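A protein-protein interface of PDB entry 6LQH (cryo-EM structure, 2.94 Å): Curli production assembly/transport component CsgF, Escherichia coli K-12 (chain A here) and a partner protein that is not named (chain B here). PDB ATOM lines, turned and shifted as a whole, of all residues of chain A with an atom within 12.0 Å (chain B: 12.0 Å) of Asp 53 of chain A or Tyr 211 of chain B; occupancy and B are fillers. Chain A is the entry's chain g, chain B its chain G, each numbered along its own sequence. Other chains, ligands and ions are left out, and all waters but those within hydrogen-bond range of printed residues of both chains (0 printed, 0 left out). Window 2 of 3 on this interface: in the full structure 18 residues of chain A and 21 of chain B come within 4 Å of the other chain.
The side-chain hydroxyl (OH) of Tyr 51 of chain A lies within hydrogen-bond range of the backbone carbonyl oxygen (O) of Ile 209 of chain B (3.3 Å).
Among the printed residues, pairs that only touch across the chains: Tyr 51 of chain A with Phe 208 of chain B, Tyr 51 of chain A with Asp 210 of chain B, Ala 45 of chain A with Phe 206 of chain B, Asp 53 of chain A with Tyr 211 of chain B, Gln 48 of chain A with Phe 159 of chain B, Asn 49 of chain A with Phe 208 of chain B, Lys 52 of chain A with Tyr 211 of chain B, Ala 45 of chain A with Phe 208 of chain B, Tyr 51 of chain A with Tyr 211 of chain B, Asn 49 of chain A with Tyr 211 of chain B and Gln 46 of chain A with Phe 208 of chain B.
Leu 42 of chain A touches none of the printed residues of chain B. Of the printed residues of chain B, Ala 45 of chain A touches Phe 206 (3.1 Å) and Phe 208 (3.4 Å). Of chain B, only Phe 208, Ile 209, Asp 210 and Tyr 211 come within 4 Å of Tyr 51 of chain A. Asp 53 of chain A touches one residue of chain B. Of the printed residues of chain A, Phe 159 of chain B touches Gln 48. Printed residues of chain A within 4 Å of Phe 206 of chain B: Ala 45 (3.1 Å). Phe 208 of chain B touches just these residues of chain A: Ala 45 (3.4 Å), Gln 46 (3.96 Å), Asn 49 (3.2 Å) and Tyr 51 (3.0 Å). Tyr 211 of chain B touches just these residues of chain A: Asn 49, Tyr 51, Lys 52 and Asp 53. No residue of chain A comes within 4 Å of Gln 212 of chain B. Leu 215 of chain B touches none of the printed residues of chain A. The nearest residue of chain B that does not touch Asp 53 of chain A is Gln 212 of chain B (5.5 Å). The nearest printed residue of chain B that does not touch Asn 49 of chain A is Asp 210 of chain B (4.1 Å).
Of the 11 printed residues of chain B, 6 touch a printed residue of chain A. Hydrophobic or aromatic side chains of chain A that line the printed part of chain B: Ala 45 and Tyr 51. Among the printed residues, no Asp or Glu carboxylate lies within 4 Å of a Lys or Arg side-chain nitrogen of the other chain.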
ATOM      1  N   LEU A  42      32.630  32.597  11.051  1.00  0.00           N
ATOM      2  CA  LEU A  42      33.213  31.475  11.776  1.00  0.00           C
ATOM      3  C   LEU A  42      33.264  31.743  13.273  1.00  0.00           C
ATOM      4  O   LEU A  42      33.058  30.825  14.073  1.00  0.00           O
ATOM      5  CB  LEU A  42      34.608  31.161  11.240  1.00  0.00           C
ATOM      6  CG  LEU A  42      35.309  29.998  11.942  1.00  0.00           C
ATOM      7  CD1 LEU A  42      34.995  28.691  11.247  1.00  0.00           C
ATOM      8  CD2 LEU A  42      36.799  30.234  12.002  1.00  0.00           C
ATOM      9  N   ALA A  45      29.777  31.302  14.614  1.00  0.00           N
ATOM     10  CA  ALA A  45      29.439  29.886  14.622  1.00  0.00           C
ATOM     11  C   ALA A  45      30.191  29.124  15.698  1.00  0.00           C
ATOM     12  O   ALA A  45      29.698  28.099  16.182  1.00  0.00           O
ATOM     13  CB  ALA A  45      29.730  29.262  13.255  1.00  0.00           C
ATOM     14  N   GLN A  46      31.374  29.600  16.081  1.00  0.00           N
ATOM     15  CA  GLN A  46      32.111  29.023  17.195  1.00  0.00           C
ATOM     16  C   GLN A  46      31.649  29.558  18.539  1.00  0.00           C
ATOM     17  O   GLN A  46      31.825  28.880  19.556  1.00  0.00           O
ATOM     18  CB  GLN A  46      33.610  29.288  17.034  1.00  0.00           C
ATOM     19  CG  GLN A  46      34.274  28.460  15.954  1.00  0.00           C
ATOM     20  CD  GLN A  46      34.658  27.074  16.430  1.00  0.00           C
ATOM     21  OE1 GLN A  46      34.163  26.591  17.447  1.00  0.00           O
ATOM     22  NE2 GLN A  46      35.550  26.425  15.693  1.00  0.00           N
ATOM     23  N   ALA A  47      31.070  30.757  18.566  1.00  0.00           N
ATOM     24  CA  ALA A  47      30.461  31.284  19.775  1.00  0.00           C
ATOM     25  C   ALA A  47      29.189  30.543  20.152  1.00  0.00           C
ATOM     26  O   ALA A  47      28.729  30.671  21.290  1.00  0.00           O
ATOM     27  CB  ALA A  47      30.158  32.773  19.605  1.00  0.00           C
ATOM     28  N   GLN A  48      28.620  29.776  19.226  1.00  0.00           N
ATOM     29  CA  GLN A  48      27.443  28.964  19.484  1.00  0.00           C
ATOM     30  C   GLN A  48      27.706  27.477  19.332  1.00  0.00           C
ATOM     31  O   GLN A  48      26.762  26.685  19.420  1.00  0.00           O
ATOM     32  CB  GLN A  48      26.301  29.368  18.547  1.00  0.00           C
ATOM     33  CG  GLN A  48      26.095  30.853  18.431  1.00  0.00           C
ATOM     34  CD  GLN A  48      24.986  31.194  17.473  1.00  0.00           C
ATOM     35  OE1 GLN A  48      23.811  31.014  17.781  1.00  0.00           O
ATOM     36  NE2 GLN A  48      25.351  31.680  16.293  1.00  0.00           N
ATOM     37  N   ASN A  49      28.949  27.074  19.091  1.00  0.00           N
ATOM     38  CA  ASN A  49      29.276  25.662  18.936  1.00  0.00           C
ATOM     39  C   ASN A  49      29.219  24.986  20.297  1.00  0.00           C
ATOM     40  O   ASN A  49      30.156  25.094  21.093  1.00  0.00           O
ATOM     41  CB  ASN A  49      30.653  25.510  18.300  1.00  0.00           C
ATOM     42  CG  ASN A  49      31.043  24.065  18.097  1.00  0.00           C
ATOM     43  OD1 ASN A  49      30.283  23.278  17.537  1.00  0.00           O
ATOM     44  ND2 ASN A  49      32.239  23.709  18.541  1.00  0.00           N
ATOM     45  N   SER A  50      28.116  24.296  20.570  1.00  0.00           N
ATOM     46  CA  SER A  50      27.906  23.623  21.842  1.00  0.00           C
ATOM     47  C   SER A  50      28.330  22.165  21.815  1.00  0.00           C
ATOM     48  O   SER A  50      27.940  21.405  22.705  1.00  0.00           O
ATOM     49  CB  SER A  50      26.435  23.717  22.249  1.00  0.00           C
ATOM     50  OG  SER A  50      25.924  22.438  22.575  1.00  0.00           O
ATOM     51  N   TYR A  51      29.109  21.755  20.821  1.00  0.00           N
ATOM     52  CA  TYR A  51      29.543  20.373  20.704  1.00  0.00           C
ATOM     53  C   TYR A  51      30.947  20.199  21.266  1.00  0.00           C
ATOM     54  O   TYR A  51      31.788  21.096  21.188  1.00  0.00           O
ATOM     55  CB  TYR A  51      29.508  19.918  19.247  1.00  0.00           C
ATOM     56  CG  TYR A  51      28.119  19.840  18.666  1.00  0.00           C
ATOM     57  CD1 TYR A  51      27.238  18.846  19.060  1.00  0.00           C
ATOM     58  CD2 TYR A  51      27.690  20.759  17.723  1.00  0.00           C
ATOM     59  CE1 TYR A  51      25.970  18.770  18.532  1.00  0.00           C
ATOM     60  CE2 TYR A  51      26.424  20.692  17.191  1.00  0.00           C
ATOM     61  CZ  TYR A  51      25.567  19.696  17.597  1.00  0.00           C
ATOM     62  OH  TYR A  51      24.300  19.627  17.066  1.00  0.00           O
ATOM     63  N   LYS A  52      31.187  19.021  21.836  1.00  0.00           N
ATOM     64  CA  LYS A  52      32.478  18.682  22.419  1.00  0.00           C
ATOM     65  C   LYS A  52      32.934  17.322  21.908  1.00  0.00           C
ATOM     66  O   LYS A  52      32.356  16.796  20.950  1.00  0.00           O
ATOM     67  CB  LYS A  52      32.399  18.691  23.946  1.00  0.00           C
ATOM     68  N   ASP A  53      33.972  16.761  22.525  1.00  0.00           N
ATOM     69  CA  ASP A  53      34.534  15.470  22.128  1.00  0.00           C
ATOM     70  C   ASP A  53      35.116  15.563  20.725  1.00  0.00           C
ATOM     71  O   ASP A  53      36.327  15.450  20.540  1.00  0.00           O
ATOM     72  CB  ASP A  53      33.475  14.360  22.206  1.00  0.00           C
ATOM     73  CG  ASP A  53      34.050  12.970  21.990  1.00  0.00           C
ATOM     74  OD1 ASP A  53      34.794  12.760  21.011  1.00  0.00           O
ATOM     75  OD2 ASP A  53      33.750  12.077  22.808  1.00  0.00           O
ATOM     76  N   PHE B 159      19.875  30.684  16.394  1.00  0.00           N
ATOM     77  CA  PHE B 159      21.137  29.964  16.446  1.00  0.00           C
ATOM     78  C   PHE B 159      21.401  29.282  15.113  1.00  0.00           C
ATOM     79  O   PHE B 159      20.784  28.264  14.786  1.00  0.00           O
ATOM     80  CB  PHE B 159      21.088  28.973  17.611  1.00  0.00           C
ATOM     81  CG  PHE B 159      21.924  27.745  17.426  1.00  0.00           C
ATOM     82  CD1 PHE B 159      23.300  27.828  17.327  1.00  0.00           C
ATOM     83  CD2 PHE B 159      21.330  26.500  17.397  1.00  0.00           C
ATOM     84  CE1 PHE B 159      24.061  26.694  17.175  1.00  0.00           C
ATOM     85  CE2 PHE B 159      22.085  25.364  17.245  1.00  0.00           C
ATOM     86  CZ  PHE B 159      23.452  25.460  17.133  1.00  0.00           C
ATOM     87  N   PHE B 206      24.578  28.567   9.290  1.00  0.00           N
ATOM     88  CA  PHE B 206      26.017  28.500   9.515  1.00  0.00           C
ATOM     89  C   PHE B 206      26.353  27.855  10.851  1.00  0.00           C
ATOM     90  O   PHE B 206      27.326  28.244  11.498  1.00  0.00           O
ATOM     91  CB  PHE B 206      26.661  29.881   9.431  1.00  0.00           C
ATOM     92  CG  PHE B 206      28.073  29.858   8.918  1.00  0.00           C
ATOM     93  CD1 PHE B 206      28.333  29.956   7.565  1.00  0.00           C
ATOM     94  CD2 PHE B 206      29.141  29.735   9.788  1.00  0.00           C
ATOM     95  CE1 PHE B 206      29.627  29.933   7.096  1.00  0.00           C
ATOM     96  CE2 PHE B 206      30.434  29.707   9.324  1.00  0.00           C
ATOM     97  CZ  PHE B 206      30.678  29.807   7.977  1.00  0.00           C
ATOM     98  N   ARG B 207      25.564  26.890  11.297  1.00  0.00           N
ATOM     99  CA  ARG B 207      25.838  26.298  12.591  1.00  0.00           C
ATOM    100  C   ARG B 207      26.636  25.007  12.429  1.00  0.00           C
ATOM    101  O   ARG B 207      26.925  24.556  11.320  1.00  0.00           O
ATOM    102  CB  ARG B 207      24.539  26.069  13.359  1.00  0.00           C
ATOM    103  CG  ARG B 207      23.569  25.108  12.716  1.00  0.00           C
ATOM    104  CD  ARG B 207      22.273  25.085  13.506  1.00  0.00           C
ATOM    105  NE  ARG B 207      21.568  23.815  13.376  1.00  0.00           N
ATOM    106  CZ  ARG B 207      21.682  22.808  14.234  1.00  0.00           C
ATOM    107  NH1 ARG B 207      22.478  22.920  15.286  1.00  0.00           N
ATOM    108  NH2 ARG B 207      21.004  21.686  14.038  1.00  0.00           N
ATOM    109  N   PHE B 208      27.012  24.412  13.555  1.00  0.00           N
ATOM    110  CA  PHE B 208      27.739  23.152  13.574  1.00  0.00           C
ATOM    111  C   PHE B 208      26.767  21.999  13.774  1.00  0.00           C
ATOM    112  O   PHE B 208      25.844  22.086  14.587  1.00  0.00           O
ATOM    113  CB  PHE B 208      28.788  23.143  14.684  1.00  0.00           C
ATOM    114  CG  PHE B 208      30.048  23.865  14.328  1.00  0.00           C
ATOM    115  CD1 PHE B 208      30.134  25.236  14.452  1.00  0.00           C
ATOM    116  CD2 PHE B 208      31.148  23.173  13.865  1.00  0.00           C
ATOM    117  CE1 PHE B 208      31.291  25.900  14.124  1.00  0.00           C
ATOM    118  CE2 PHE B 208      32.306  23.836  13.535  1.00  0.00           C
ATOM    119  CZ  PHE B 208      32.377  25.198  13.665  1.00  0.00           C
ATOM    120  N   ILE B 209      26.978  20.924  13.023  1.00  0.00           N
ATOM    121  CA  ILE B 209      26.119  19.750  13.130  1.00  0.00           C
ATOM    122  C   ILE B 209      26.719  18.715  14.068  1.00  0.00           C
ATOM    123  O   ILE B 209      25.994  18.016  14.779  1.00  0.00           O
ATOM    124  CB  ILE B 209      25.861  19.154  11.732  1.00  0.00           C
ATOM    125  CG1 ILE B 209      25.398  20.238  10.769  1.00  0.00           C
ATOM    126  CG2 ILE B 209      24.818  18.056  11.803  1.00  0.00           C
ATOM    127  CD1 ILE B 209      24.315  21.129  11.327  1.00  0.00           C
ATOM    128  N   ASP B 210      28.043  18.608  14.079  1.00  0.00           N
ATOM    129  CA  ASP B 210      28.730  17.670  14.950  1.00  0.00           C
ATOM    130  C   ASP B 210      29.816  18.428  15.695  1.00  0.00           C
ATOM    131  O   ASP B 210      29.816  19.661  15.688  1.00  0.00           O
ATOM    132  CB  ASP B 210      29.308  16.510  14.143  1.00  0.00           C
ATOM    133  CG  ASP B 210      28.704  15.179  14.529  1.00  0.00           C
ATOM    134  OD1 ASP B 210      29.443  14.310  15.034  1.00  0.00           O
ATOM    135  OD2 ASP B 210      27.486  14.998  14.323  1.00  0.00           O
ATOM    136  N   TYR B 211      30.731  17.715  16.353  1.00  0.00           N
ATOM    137  CA  TYR B 211      31.815  18.388  17.060  1.00  0.00           C
ATOM    138  C   TYR B 211      32.587  19.310  16.126  1.00  0.00           C
ATOM    139  O   TYR B 211      32.695  20.516  16.366  1.00  0.00           O
ATOM    140  CB  TYR B 211      32.753  17.364  17.697  1.00  0.00           C
ATOM    141  CG  TYR B 211      33.977  17.994  18.326  1.00  0.00           C
ATOM    142  CD1 TYR B 211      33.867  19.135  19.108  1.00  0.00           C
ATOM    143  CD2 TYR B 211      35.237  17.455  18.132  1.00  0.00           C
ATOM    144  CE1 TYR B 211      34.974  19.718  19.681  1.00  0.00           C
ATOM    145  CE2 TYR B 211      36.353  18.029  18.705  1.00  0.00           C
ATOM    146  CZ  TYR B 211      36.217  19.162  19.479  1.00  0.00           C
ATOM    147  OH  TYR B 211      37.325  19.741  20.052  1.00  0.00           O
ATOM    148  N   GLN B 212      33.127  18.756  15.048  1.00  0.00           N
ATOM    149  CA  GLN B 212      33.932  19.501  14.094  1.00  0.00           C
ATOM    150  C   GLN B 212      33.380  19.341  12.687  1.00  0.00           C
ATOM    151  O   GLN B 212      34.107  19.041  11.741  1.00  0.00           O
ATOM    152  CB  GLN B 212      35.392  19.066  14.165  1.00  0.00           C
ATOM    153  CG  GLN B 212      36.174  19.763  15.258  1.00  0.00           C
ATOM    154  CD  GLN B 212      37.471  19.061  15.587  1.00  0.00           C
ATOM    155  OE1 GLN B 212      37.510  17.838  15.718  1.00  0.00           O
ATOM    156  NE2 GLN B 212      38.542  19.831  15.723  1.00  0.00           N
ATOM    157  N   ARG B 213      32.071  19.519  12.545  1.00  0.00           N
ATOM    158  CA  ARG B 213      31.392  19.446  11.260  1.00  0.00           C
ATOM    159  C   ARG B 213      30.509  20.676  11.119  1.00  0.00           C
ATOM    160  O   ARG B 213      29.552  20.846  11.879  1.00  0.00           O
ATOM    161  CB  ARG B 213      30.570  18.164  11.144  1.00  0.00           C
ATOM    162  CG  ARG B 213      31.387  16.896  11.272  1.00  0.00           C
ATOM    163  CD  ARG B 213      32.436  16.801  10.186  1.00  0.00           C
ATOM    164  NE  ARG B 213      33.233  15.583  10.289  1.00  0.00           N
ATOM    165  CZ  ARG B 213      34.468  15.538  10.774  1.00  0.00           C
ATOM    166  NH1 ARG B 213      35.056  16.645  11.205  1.00  0.00           N
ATOM    167  NH2 ARG B 213      35.117  14.385  10.830  1.00  0.00           N
ATOM    168  N   LEU B 214      30.836  21.529  10.160  1.00  0.00           N
ATOM    169  CA  LEU B 214      30.158  22.802   9.966  1.00  0.00           C
ATOM    170  C   LEU B 214      29.321  22.729   8.700  1.00  0.00           C
ATOM    171  O   LEU B 214      29.850  22.457   7.618  1.00  0.00           O
ATOM    172  CB  LEU B 214      31.175  23.938   9.875  1.00  0.00           C
ATOM    173  CG  LEU B 214      30.663  25.327   9.515  1.00  0.00           C
ATOM    174  CD1 LEU B 214      30.021  25.973  10.720  1.00  0.00           C
ATOM    175  CD2 LEU B 214      31.808  26.170   9.008  1.00  0.00           C
ATOM    176  N   LEU B 215      28.022  22.978   8.833  1.00  0.00           N
ATOM    177  CA  LEU B 215      27.106  23.000   7.698  1.00  0.00           C
ATOM    178  C   LEU B 215      26.724  24.439   7.384  1.00  0.00           C
ATOM    179  O   LEU B 215      26.025  25.087   8.167  1.00  0.00           O
ATOM    180  CB  LEU B 215      25.864  22.166   7.979  1.00  0.00           C
ATOM    181  CG  LEU B 215      24.770  22.272   6.927  1.00  0.00           C
ATOM    182  CD1 LEU B 215      24.370  20.891   6.491  1.00  0.00           C
ATOM    183  CD2 LEU B 215      23.579  23.008   7.486  1.00  0.00           C
